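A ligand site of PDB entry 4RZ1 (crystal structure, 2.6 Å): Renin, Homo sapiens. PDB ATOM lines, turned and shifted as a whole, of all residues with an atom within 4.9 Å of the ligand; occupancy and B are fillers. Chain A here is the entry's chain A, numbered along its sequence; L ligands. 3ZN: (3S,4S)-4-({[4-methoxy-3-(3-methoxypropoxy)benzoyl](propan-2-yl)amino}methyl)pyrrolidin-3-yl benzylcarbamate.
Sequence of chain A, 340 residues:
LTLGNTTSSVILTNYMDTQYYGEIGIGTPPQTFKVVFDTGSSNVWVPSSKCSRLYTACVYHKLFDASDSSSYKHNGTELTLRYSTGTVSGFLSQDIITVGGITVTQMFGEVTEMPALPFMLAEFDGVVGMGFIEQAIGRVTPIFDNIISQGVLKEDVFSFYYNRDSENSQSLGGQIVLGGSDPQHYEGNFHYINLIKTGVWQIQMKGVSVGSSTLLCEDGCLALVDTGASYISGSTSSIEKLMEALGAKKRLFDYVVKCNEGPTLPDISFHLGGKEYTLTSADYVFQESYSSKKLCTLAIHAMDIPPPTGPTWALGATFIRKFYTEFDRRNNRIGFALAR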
ATOM      1  N   THR A  18     -29.154  24.473  10.134  1.00  0.00           N
ATOM      2  CA  THR A  18     -27.694  24.543  10.074  1.00  0.00           C
ATOM      3  C   THR A  18     -27.142  23.576   9.045  1.00  0.00           C
ATOM      4  O   THR A  18     -26.082  23.827   8.504  1.00  0.00           O
ATOM      5  CB  THR A  18     -27.035  24.353  11.457  1.00  0.00           C
ATOM      6  OG1 THR A  18     -27.426  23.109  12.029  1.00  0.00           O
ATOM      7  CG2 THR A  18     -27.339  25.480  12.412  1.00  0.00           C
ATOM      8  N   GLN A  19     -27.843  22.457   8.792  1.00  0.00           N
ATOM      9  CA  GLN A  19     -27.333  21.460   7.829  1.00  0.00           C
ATOM     10  C   GLN A  19     -28.400  21.119   6.807  1.00  0.00           C
ATOM     11  O   GLN A  19     -29.528  20.812   7.196  1.00  0.00           O
ATOM     12  CB  GLN A  19     -26.833  20.201   8.560  1.00  0.00           C
ATOM     13  CG  GLN A  19     -25.781  20.473   9.634  1.00  0.00           C
ATOM     14  CD  GLN A  19     -25.252  19.215  10.277  1.00  0.00           C
ATOM     15  OE1 GLN A  19     -25.089  18.178   9.639  1.00  0.00           O
ATOM     16  NE2 GLN A  19     -24.934  19.301  11.566  1.00  0.00           N
ATOM     17  N   TYR A  20     -28.059  21.172   5.507  1.00  0.00           N
ATOM     18  CA  TYR A  20     -28.959  20.823   4.404  1.00  0.00           C
ATOM     19  C   TYR A  20     -28.268  19.776   3.577  1.00  0.00           C
ATOM     20  O   TYR A  20     -27.138  19.998   3.105  1.00  0.00           O
ATOM     21  CB  TYR A  20     -29.308  22.035   3.524  1.00  0.00           C
ATOM     22  CG  TYR A  20     -30.134  23.087   4.226  1.00  0.00           C
ATOM     23  CD1 TYR A  20     -29.545  24.020   5.068  1.00  0.00           C
ATOM     24  CD2 TYR A  20     -31.511  23.160   4.041  1.00  0.00           C
ATOM     25  CE1 TYR A  20     -30.299  24.991   5.720  1.00  0.00           C
ATOM     26  CE2 TYR A  20     -32.273  24.136   4.658  1.00  0.00           C
ATOM     27  CZ  TYR A  20     -31.658  25.056   5.496  1.00  0.00           C
ATOM     28  OH  TYR A  20     -32.400  26.053   6.082  1.00  0.00           O
ATOM     29  N   VAL A  36     -23.837  16.716   1.378  1.00  0.00           N
ATOM     30  CA  VAL A  36     -24.025  18.154   1.253  1.00  0.00           C
ATOM     31  C   VAL A  36     -23.659  18.508  -0.199  1.00  0.00           C
ATOM     32  O   VAL A  36     -22.635  18.044  -0.715  1.00  0.00           O
ATOM     33  CB  VAL A  36     -23.136  18.946   2.240  1.00  0.00           C
ATOM     34  CG1 VAL A  36     -23.168  20.436   1.933  1.00  0.00           C
ATOM     35  CG2 VAL A  36     -23.534  18.683   3.684  1.00  0.00           C
ATOM     36  N   ASP A  38     -22.237  21.218  -2.076  1.00  0.00           N
ATOM     37  CA  ASP A  38     -21.348  22.302  -1.663  1.00  0.00           C
ATOM     38  C   ASP A  38     -20.733  23.105  -2.812  1.00  0.00           C
ATOM     39  O   ASP A  38     -19.840  22.603  -3.478  1.00  0.00           O
ATOM     40  CB  ASP A  38     -20.256  21.694  -0.752  1.00  0.00           C
ATOM     41  CG  ASP A  38     -19.251  22.625  -0.139  1.00  0.00           C
ATOM     42  OD1 ASP A  38     -19.496  23.842  -0.148  1.00  0.00           O
ATOM     43  OD2 ASP A  38     -18.254  22.140   0.422  1.00  0.00           O
ATOM     44  N   GLY A  40     -18.837  25.634  -2.355  1.00  0.00           N
ATOM     45  CA  GLY A  40     -17.548  26.035  -1.822  1.00  0.00           C
ATOM     46  C   GLY A  40     -16.453  25.011  -1.985  1.00  0.00           C
ATOM     47  O   GLY A  40     -15.341  25.242  -1.513  1.00  0.00           O
ATOM     48  N   SER A  41     -16.737  23.873  -2.644  1.00  0.00           N
ATOM     49  CA  SER A  41     -15.744  22.806  -2.867  1.00  0.00           C
ATOM     50  C   SER A  41     -16.044  22.042  -4.168  1.00  0.00           C
ATOM     51  O   SER A  41     -17.131  22.193  -4.717  1.00  0.00           O
ATOM     52  CB  SER A  41     -15.586  21.892  -1.662  1.00  0.00           C
ATOM     53  OG  SER A  41     -16.727  21.073  -1.478  1.00  0.00           O
ATOM     54  N   TRP A  45     -16.790  13.227  -1.881  1.00  0.00           N
ATOM     55  CA  TRP A  45     -16.241  12.260  -0.938  1.00  0.00           C
ATOM     56  C   TRP A  45     -17.332  11.682  -0.082  1.00  0.00           C
ATOM     57  O   TRP A  45     -18.322  12.364   0.176  1.00  0.00           O
ATOM     58  CB  TRP A  45     -15.062  12.800  -0.096  1.00  0.00           C
ATOM     59  CG  TRP A  45     -15.413  13.856   0.920  1.00  0.00           C
ATOM     60  CD1 TRP A  45     -15.354  15.198   0.745  1.00  0.00           C
ATOM     61  CD2 TRP A  45     -15.849  13.643   2.277  1.00  0.00           C
ATOM     62  NE1 TRP A  45     -15.669  15.844   1.919  1.00  0.00           N
ATOM     63  CE2 TRP A  45     -16.006  14.918   2.866  1.00  0.00           C
ATOM     64  CE3 TRP A  45     -16.141  12.503   3.046  1.00  0.00           C
ATOM     65  CZ2 TRP A  45     -16.450  15.076   4.193  1.00  0.00           C
ATOM     66  CZ3 TRP A  45     -16.531  12.661   4.363  1.00  0.00           C
ATOM     67  CH2 TRP A  45     -16.718  13.936   4.908  1.00  0.00           C
ATOM     68  N   ARG A  82      -8.822  20.041   3.038  1.00  0.00           N
ATOM     69  CA  ARG A  82      -8.787  20.916   4.197  1.00  0.00           C
ATOM     70  C   ARG A  82      -9.898  21.943   4.086  1.00  0.00           C
ATOM     71  O   ARG A  82     -10.113  22.528   3.033  1.00  0.00           O
ATOM     72  CB  ARG A  82      -7.425  21.612   4.322  1.00  0.00           C
ATOM     73  CG  ARG A  82      -6.307  20.719   4.832  1.00  0.00           C
ATOM     74  CD  ARG A  82      -4.944  21.042   4.170  1.00  0.00           C
ATOM     75  NE  ARG A  82      -3.948  19.977   4.415  1.00  0.00           N
ATOM     76  CZ  ARG A  82      -3.232  19.343   3.474  1.00  0.00           C
ATOM     77  NH1 ARG A  82      -3.358  19.670   2.197  1.00  0.00           N
ATOM     78  NH2 ARG A  82      -2.396  18.375   3.826  1.00  0.00           N
ATOM     79  N   TYR A  83     -10.582  22.178   5.189  1.00  0.00           N
ATOM     80  CA  TYR A  83     -11.653  23.157   5.306  1.00  0.00           C
ATOM     81  C   TYR A  83     -11.369  24.039   6.512  1.00  0.00           C
ATOM     82  O   TYR A  83     -10.435  23.789   7.264  1.00  0.00           O
ATOM     83  CB  TYR A  83     -12.982  22.428   5.480  1.00  0.00           C
ATOM     84  CG  TYR A  83     -13.315  21.393   4.427  1.00  0.00           C
ATOM     85  CD1 TYR A  83     -13.618  21.781   3.119  1.00  0.00           C
ATOM     86  CD2 TYR A  83     -13.481  20.053   4.762  1.00  0.00           C
ATOM     87  CE1 TYR A  83     -14.048  20.850   2.170  1.00  0.00           C
ATOM     88  CE2 TYR A  83     -13.883  19.114   3.818  1.00  0.00           C
ATOM     89  CZ  TYR A  83     -14.169  19.519   2.525  1.00  0.00           C
ATOM     90  OH  TYR A  83     -14.576  18.616   1.586  1.00  0.00           O
ATOM     91  N   SER A  84     -12.165  25.078   6.708  1.00  0.00           N
ATOM     92  CA  SER A  84     -12.053  26.011   7.823  1.00  0.00           C
ATOM     93  C   SER A  84     -12.404  25.341   9.172  1.00  0.00           C
ATOM     94  O   SER A  84     -12.018  25.866  10.218  1.00  0.00           O
ATOM     95  CB  SER A  84     -12.981  27.199   7.581  1.00  0.00           C
ATOM     96  OG  SER A  84     -12.510  28.421   8.122  1.00  0.00           O
ATOM     97  N   THR A  85     -13.133  24.202   9.156  1.00  0.00           N
ATOM     98  CA  THR A  85     -13.699  23.493  10.320  1.00  0.00           C
ATOM     99  C   THR A  85     -12.936  22.247  10.735  1.00  0.00           C
ATOM    100  O   THR A  85     -13.041  21.787  11.880  1.00  0.00           O
ATOM    101  CB  THR A  85     -15.168  23.110  10.014  1.00  0.00           C
ATOM    102  OG1 THR A  85     -15.226  22.543   8.700  1.00  0.00           O
ATOM    103  CG2 THR A  85     -16.122  24.310  10.105  1.00  0.00           C
ATOM    104  N   PRO A 118     -15.264  18.355  13.069  1.00  0.00           N
ATOM    105  CA  PRO A 118     -16.703  18.499  13.364  1.00  0.00           C
ATOM    106  C   PRO A 118     -17.628  17.345  12.947  1.00  0.00           C
ATOM    107  O   PRO A 118     -18.836  17.457  13.142  1.00  0.00           O
ATOM    108  CB  PRO A 118     -17.049  19.755  12.552  1.00  0.00           C
ATOM    109  CG  PRO A 118     -16.194  19.591  11.270  1.00  0.00           C
ATOM    110  CD  PRO A 118     -14.962  18.806  11.694  1.00  0.00           C
ATOM    111  N   PHE A 119     -17.092  16.237  12.415  1.00  0.00           N
ATOM    112  CA  PHE A 119     -17.897  15.184  11.804  1.00  0.00           C
ATOM    113  C   PHE A 119     -18.771  14.371  12.777  1.00  0.00           C
ATOM    114  O   PHE A 119     -19.740  13.778  12.302  1.00  0.00           O
ATOM    115  CB  PHE A 119     -17.061  14.301  10.898  1.00  0.00           C
ATOM    116  CG  PHE A 119     -16.501  15.164   9.787  1.00  0.00           C
ATOM    117  CD1 PHE A 119     -17.321  15.647   8.763  1.00  0.00           C
ATOM    118  CD2 PHE A 119     -15.186  15.612   9.821  1.00  0.00           C
ATOM    119  CE1 PHE A 119     -16.827  16.513   7.791  1.00  0.00           C
ATOM    120  CE2 PHE A 119     -14.697  16.515   8.855  1.00  0.00           C
ATOM    121  CZ  PHE A 119     -15.522  16.940   7.845  1.00  0.00           C
ATOM    122  N   LEU A 121     -20.776  15.879  14.682  1.00  0.00           N
ATOM    123  CA  LEU A 121     -21.920  16.790  14.652  1.00  0.00           C
ATOM    124  C   LEU A 121     -22.593  16.775  13.292  1.00  0.00           C
ATOM    125  O   LEU A 121     -23.672  17.349  13.137  1.00  0.00           O
ATOM    126  CB  LEU A 121     -21.493  18.215  14.962  1.00  0.00           C
ATOM    127  CG  LEU A 121     -20.587  18.440  16.162  1.00  0.00           C
ATOM    128  CD1 LEU A 121     -19.535  19.469  15.819  1.00  0.00           C
ATOM    129  CD2 LEU A 121     -21.368  18.813  17.388  1.00  0.00           C
ATOM    130  N   ALA A 122     -21.948  16.130  12.300  1.00  0.00           N
ATOM    131  CA  ALA A 122     -22.461  16.013  10.955  1.00  0.00           C
ATOM    132  C   ALA A 122     -23.609  15.010  10.870  1.00  0.00           C
ATOM    133  O   ALA A 122     -23.497  13.881  11.371  1.00  0.00           O
ATOM    134  CB  ALA A 122     -21.355  15.637   9.989  1.00  0.00           C
ATOM    135  N   PHE A 124     -24.960  14.618   7.749  1.00  0.00           N
ATOM    136  CA  PHE A 124     -24.602  14.136   6.429  1.00  0.00           C
ATOM    137  C   PHE A 124     -23.394  13.211   6.596  1.00  0.00           C
ATOM    138  O   PHE A 124     -22.635  13.378   7.567  1.00  0.00           O
ATOM    139  CB  PHE A 124     -24.221  15.324   5.522  1.00  0.00           C
ATOM    140  CG  PHE A 124     -23.155  16.243   6.066  1.00  0.00           C
ATOM    141  CD1 PHE A 124     -23.473  17.203   7.016  1.00  0.00           C
ATOM    142  CD2 PHE A 124     -21.852  16.167   5.618  1.00  0.00           C
ATOM    143  CE1 PHE A 124     -22.487  18.078   7.501  1.00  0.00           C
ATOM    144  CE2 PHE A 124     -20.857  17.030   6.119  1.00  0.00           C
ATOM    145  CZ  PHE A 124     -21.192  17.994   7.046  1.00  0.00           C
ATOM    146  N   VAL A 127     -19.746  14.746   1.052  1.00  0.00           N
ATOM    147  CA  VAL A 127     -19.865  15.989   0.295  1.00  0.00           C
ATOM    148  C   VAL A 127     -19.901  15.694  -1.202  1.00  0.00           C
ATOM    149  O   VAL A 127     -19.273  14.752  -1.663  1.00  0.00           O
ATOM    150  CB  VAL A 127     -18.697  16.956   0.657  1.00  0.00           C
ATOM    151  CG1 VAL A 127     -18.762  18.268  -0.119  1.00  0.00           C
ATOM    152  CG2 VAL A 127     -18.649  17.226   2.165  1.00  0.00           C
ATOM    153  N   GLN A 135     -10.645  24.341  -8.453  1.00  0.00           N
ATOM    154  CA  GLN A 135     -10.538  24.192  -7.002  1.00  0.00           C
ATOM    155  C   GLN A 135     -10.519  22.712  -6.547  1.00  0.00           C
ATOM    156  O   GLN A 135     -10.450  22.456  -5.345  1.00  0.00           O
ATOM    157  CB  GLN A 135     -11.664  24.959  -6.281  1.00  0.00           C
ATOM    158  CG  GLN A 135     -11.651  26.487  -6.419  1.00  0.00           C
ATOM    159  CD  GLN A 135     -10.558  27.254  -5.732  1.00  0.00           C
ATOM    160  OE1 GLN A 135      -9.427  27.345  -6.224  1.00  0.00           O
ATOM    161  NE2 GLN A 135     -10.902  27.917  -4.621  1.00  0.00           N
ATOM    162  N   TYR A 162     -33.422  26.504  -0.054  1.00  0.00           N
ATOM    163  CA  TYR A 162     -33.229  26.098   1.347  1.00  0.00           C
ATOM    164  C   TYR A 162     -34.401  26.644   2.118  1.00  0.00           C
ATOM    165  O   TYR A 162     -34.543  27.862   2.263  1.00  0.00           O
ATOM    166  CB  TYR A 162     -31.918  26.690   1.929  1.00  0.00           C
ATOM    167  CG  TYR A 162     -30.631  25.967   1.608  1.00  0.00           C
ATOM    168  CD1 TYR A 162     -30.631  24.813   0.820  1.00  0.00           C
ATOM    169  CD2 TYR A 162     -29.413  26.413   2.109  1.00  0.00           C
ATOM    170  CE1 TYR A 162     -29.452  24.143   0.528  1.00  0.00           C
ATOM    171  CE2 TYR A 162     -28.216  25.747   1.804  1.00  0.00           C
ATOM    172  CZ  TYR A 162     -28.257  24.593   1.038  1.00  0.00           C
ATOM    173  OH  TYR A 162     -27.114  23.911   0.761  1.00  0.00           O
ATOM    174  N   LEU A 224     -18.204  35.075  -1.265  1.00  0.00           N
ATOM    175  CA  LEU A 224     -18.247  33.701  -1.730  1.00  0.00           C
ATOM    176  C   LEU A 224     -19.703  33.152  -1.495  1.00  0.00           C
ATOM    177  O   LEU A 224     -20.230  33.334  -0.398  1.00  0.00           O
ATOM    178  CB  LEU A 224     -17.193  32.911  -0.938  1.00  0.00           C
ATOM    179  CG  LEU A 224     -16.924  31.496  -1.377  1.00  0.00           C
ATOM    180  CD1 LEU A 224     -15.987  31.445  -2.585  1.00  0.00           C
ATOM    181  CD2 LEU A 224     -16.358  30.713  -0.230  1.00  0.00           C
ATOM    182  N   ASP A 226     -21.560  30.139  -0.815  1.00  0.00           N
ATOM    183  CA  ASP A 226     -21.278  28.781  -0.320  1.00  0.00           C
ATOM    184  C   ASP A 226     -22.509  28.014   0.254  1.00  0.00           C
ATOM    185  O   ASP A 226     -22.855  28.171   1.431  1.00  0.00           O
ATOM    186  CB  ASP A 226     -20.149  28.849   0.724  1.00  0.00           C
ATOM    187  CG  ASP A 226     -19.483  27.550   1.084  1.00  0.00           C
ATOM    188  OD1 ASP A 226     -19.864  26.512   0.521  1.00  0.00           O
ATOM    189  OD2 ASP A 226     -18.541  27.575   1.902  1.00  0.00           O
ATOM    190  N   THR A 227     -23.099  27.131  -0.533  1.00  0.00           N
ATOM    191  CA  THR A 227     -24.245  26.301  -0.148  1.00  0.00           C
ATOM    192  C   THR A 227     -23.883  25.263   0.941  1.00  0.00           C
ATOM    193  O   THR A 227     -24.798  24.724   1.566  1.00  0.00           O
ATOM    194  CB  THR A 227     -24.788  25.562  -1.378  1.00  0.00           C
ATOM    195  OG1 THR A 227     -23.765  24.711  -1.890  1.00  0.00           O
ATOM    196  CG2 THR A 227     -25.288  26.511  -2.476  1.00  0.00           C
ATOM    197  N   GLY A 228     -22.591  24.994   1.143  1.00  0.00           N
ATOM    198  CA  GLY A 228     -22.115  24.034   2.136  1.00  0.00           C
ATOM    199  C   GLY A 228     -21.843  24.637   3.495  1.00  0.00           C
ATOM    200  O   GLY A 228     -21.424  23.923   4.424  1.00  0.00           O
ATOM    201  N   ALA A 229     -22.042  25.950   3.620  1.00  0.00           N
ATOM    202  CA  ALA A 229     -21.826  26.698   4.849  1.00  0.00           C
ATOM    203  C   ALA A 229     -23.192  27.025   5.470  1.00  0.00           C
ATOM    204  O   ALA A 229     -24.158  27.308   4.747  1.00  0.00           O
ATOM    205  CB  ALA A 229     -21.044  27.967   4.549  1.00  0.00           C
ATOM    206  N   SER A 230     -23.260  26.951   6.808  1.00  0.00           N
ATOM    207  CA  SER A 230     -24.438  27.202   7.608  1.00  0.00           C
ATOM    208  C   SER A 230     -24.758  28.663   7.743  1.00  0.00           C
ATOM    209  O   SER A 230     -25.932  29.025   7.831  1.00  0.00           O
ATOM    210  CB  SER A 230     -24.258  26.654   9.005  1.00  0.00           C
ATOM    211  OG  SER A 230     -23.927  25.295   8.946  1.00  0.00           O
ATOM    212  N   MET A 303     -14.868  34.108  10.129  1.00  0.00           N
ATOM    213  CA  MET A 303     -14.155  33.042   9.452  1.00  0.00           C
ATOM    214  C   MET A 303     -13.069  33.657   8.602  1.00  0.00           C
ATOM    215  O   MET A 303     -13.365  34.250   7.554  1.00  0.00           O
ATOM    216  CB  MET A 303     -15.106  32.179   8.625  1.00  0.00           C
ATOM    217  CG  MET A 303     -14.466  30.962   8.022  1.00  0.00           C
ATOM    218  SD  MET A 303     -15.758  29.767   7.625  1.00  0.00           S
ATOM    219  CE  MET A 303     -15.983  28.979   9.268  1.00  0.00           C
ATOM    220  N   ILE A 305     -10.687  33.465   5.975  1.00  0.00           N
ATOM    221  CA  ILE A 305     -10.409  32.672   4.788  1.00  0.00           C
ATOM    222  C   ILE A 305      -9.088  33.197   4.223  1.00  0.00           C
ATOM    223  O   ILE A 305      -8.923  34.423   4.100  1.00  0.00           O
ATOM    224  CB  ILE A 305     -11.601  32.693   3.802  1.00  0.00           C
ATOM    225  CG1 ILE A 305     -12.815  31.926   4.409  1.00  0.00           C
ATOM    226  CG2 ILE A 305     -11.210  32.122   2.435  1.00  0.00           C
ATOM    227  CD1 ILE A 305     -14.235  32.353   3.951  1.00  0.00           C
ATOM    228  N   THR A 309      -8.356  32.729  -2.302  1.00  0.00           N
ATOM    229  CA  THR A 309      -9.814  32.956  -2.152  1.00  0.00           C
ATOM    230  C   THR A 309     -10.123  34.141  -1.200  1.00  0.00           C
ATOM    231  O   THR A 309     -10.882  35.032  -1.571  1.00  0.00           O
ATOM    232  CB  THR A 309     -10.567  31.657  -1.762  1.00  0.00           C
ATOM    233  OG1 THR A 309     -10.245  30.624  -2.691  1.00  0.00           O
ATOM    234  CG2 THR A 309     -12.097  31.854  -1.731  1.00  0.00           C
ATOM    235  N   ALA A 317     -26.134  29.256   4.185  1.00  0.00           N
ATOM    236  CA  ALA A 317     -27.578  28.936   4.321  1.00  0.00           C
ATOM    237  C   ALA A 317     -28.436  30.093   4.857  1.00  0.00           C
ATOM    238  O   ALA A 317     -29.579  30.217   4.427  1.00  0.00           O
ATOM    239  CB  ALA A 317     -27.787  27.680   5.142  1.00  0.00           C
HETATM  240  C2  3ZN L   1     -18.274  24.471   2.977  1.00  0.00           C
HETATM  241  C3  3ZN L   1     -17.147  23.957   3.891  1.00  0.00           C
HETATM  242  C11 3ZN L   1     -17.945  19.406   4.716  1.00  0.00           C
HETATM  243  C12 3ZN L   1     -17.967  22.275   6.429  1.00  0.00           C
HETATM  244  C13 3ZN L   1     -18.906  21.764   7.499  1.00  0.00           C
HETATM  245  C14 3ZN L   1     -18.459  21.039   8.618  1.00  0.00           C
HETATM  246  C15 3ZN L   1     -20.770  20.861   9.456  1.00  0.00           C
HETATM  247  C16 3ZN L   1     -21.217  21.615   8.346  1.00  0.00           C
HETATM  248  C17 3ZN L   1     -19.383  20.577   9.590  1.00  0.00           C
HETATM  249  C18 3ZN L   1     -20.280  22.076   7.385  1.00  0.00           C
HETATM  250  C21 3ZN L   1     -21.437  19.833  11.638  1.00  0.00           C
HETATM  251  C23 3ZN L   1     -23.241  22.533   7.171  1.00  0.00           C
HETATM  252  C24 3ZN L   1     -23.643  21.547   6.039  1.00  0.00           C
HETATM  253  C25 3ZN L   1     -24.329  22.281   4.845  1.00  0.00           C
HETATM  254  C27 3ZN L   1     -25.652  24.307   4.853  1.00  0.00           C
HETATM  255  C28 3ZN L   1     -14.427  26.329   4.130  1.00  0.00           C
HETATM  256  N1  3ZN L   1     -17.603  24.732   1.693  1.00  0.00           N
HETATM  257  C4  3ZN L   1     -15.841  24.596   3.352  1.00  0.00           C
HETATM  258  C5  3ZN L   1     -16.214  25.157   1.968  1.00  0.00           C
HETATM  259  C6  3ZN L   1     -16.989  22.443   4.157  1.00  0.00           C
HETATM  260  O7  3ZN L   1     -15.463  25.542   4.369  1.00  0.00           O
HETATM  261  N8  3ZN L   1     -17.975  21.859   5.093  1.00  0.00           N
HETATM  262  C9  3ZN L   1     -18.806  20.693   4.673  1.00  0.00           C
HETATM  263  C10 3ZN L   1     -19.547  20.854   3.322  1.00  0.00           C
HETATM  264  O19 3ZN L   1     -17.260  23.180   6.850  1.00  0.00           O
HETATM  265  O20 3ZN L   1     -21.755  20.466  10.377  1.00  0.00           O
HETATM  266  O22 3ZN L   1     -22.593  21.873   8.277  1.00  0.00           O
HETATM  267  O26 3ZN L   1     -25.547  22.946   5.280  1.00  0.00           O
HETATM  268  N29 3ZN L   1     -14.812  27.587   3.806  1.00  0.00           N
HETATM  269  O30 3ZN L   1     -13.281  25.943   4.270  1.00  0.00           O
HETATM  270  C31 3ZN L   1     -13.815  28.603   3.500  1.00  0.00           C
HETATM  271  C32 3ZN L   1     -13.297  28.454   2.052  1.00  0.00           C
HETATM  272  C33 3ZN L   1     -11.921  28.596   1.762  1.00  0.00           C
HETATM  273  C34 3ZN L   1     -12.356  28.242  -0.591  1.00  0.00           C
HETATM  274  C35 3ZN L   1     -13.732  28.072  -0.311  1.00  0.00           C
HETATM  275  C36 3ZN L   1     -11.441  28.506   0.439  1.00  0.00           C
HETATM  276  C37 3ZN L   1     -14.207  28.173   1.007  1.00  0.00           C
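The side-chain carboxylate (OD1) of Asp 38 is in salt-bridge range of a nitrogen (N1) of the ligand (2.8 Å).
N of Ser 84 is in hydrogen-bond range of O30 of the ligand.
OG1 of Thr 85 lies within hydrogen-bond range of O19 of the ligand, 2.8 Å away.
N1 of the ligand lies within salt-bridge range of OD2 of Asp 226.
An oxygen (O26) of the ligand lies within hydrogen-bond range of the backbone NH of Tyr 20 (3.1 Å).
N of Gly 40 lies within hydrogen-bond range of OD1 of Asp 38, at 2.9 Å.
The backbone NH (N) of Gly 40 is in hydrogen-bond range of the side-chain carboxylate (OD1) of Asp 226 (3.2 Å).
The backbone carbonyl oxygen of Thr 18 is in hydrogen-bond range of the side-chain hydroxyl of Ser 230 (2.6 Å).
The backbone carbonyl oxygen (O) of Ala 229 lies within hydrogen-bond range of the backbone NH (N) of Ala 317.
NE1 of Trp 45 lies within hydrogen-bond range of OH of Tyr 83 (3.0 Å).
OH of Tyr 162 sits at hydrogen-bond distance from O of Thr 227.
NE2 of Gln 19 sits at hydrogen-bond distance from O of Leu 121, at 2.8 Å.
The side-chain hydroxyl (OG1) of Thr 309 is in hydrogen-bond range of the side-chain amide nitrogen (NE2) of Gln 135 (3.4 Å).
The backbone carbonyl oxygen (O) of Thr 18 sits close to an oxygen (O26) of the ligand (3.4 Å).
Residues that only touch the ligand: Ala 229 (3.4 Å), Ser 230 (3.4 Å), Gly 228 (3.4 Å), Tyr 83 (3.4 Å), Thr 227 (3.4 Å), Val 127 (3.4 Å), Gln 19 (3.4 Å), Gly 40 (3.5 Å), Leu 224 (3.6 Å), Ile 305 (3.6 Å), Val 36 (3.6 Å), Leu 121 (3.7 Å), Pro 118 (3.7 Å), Phe 124 (3.8 Å), Ala 122 (3.8 Å) and Thr 309 (3.8 Å).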
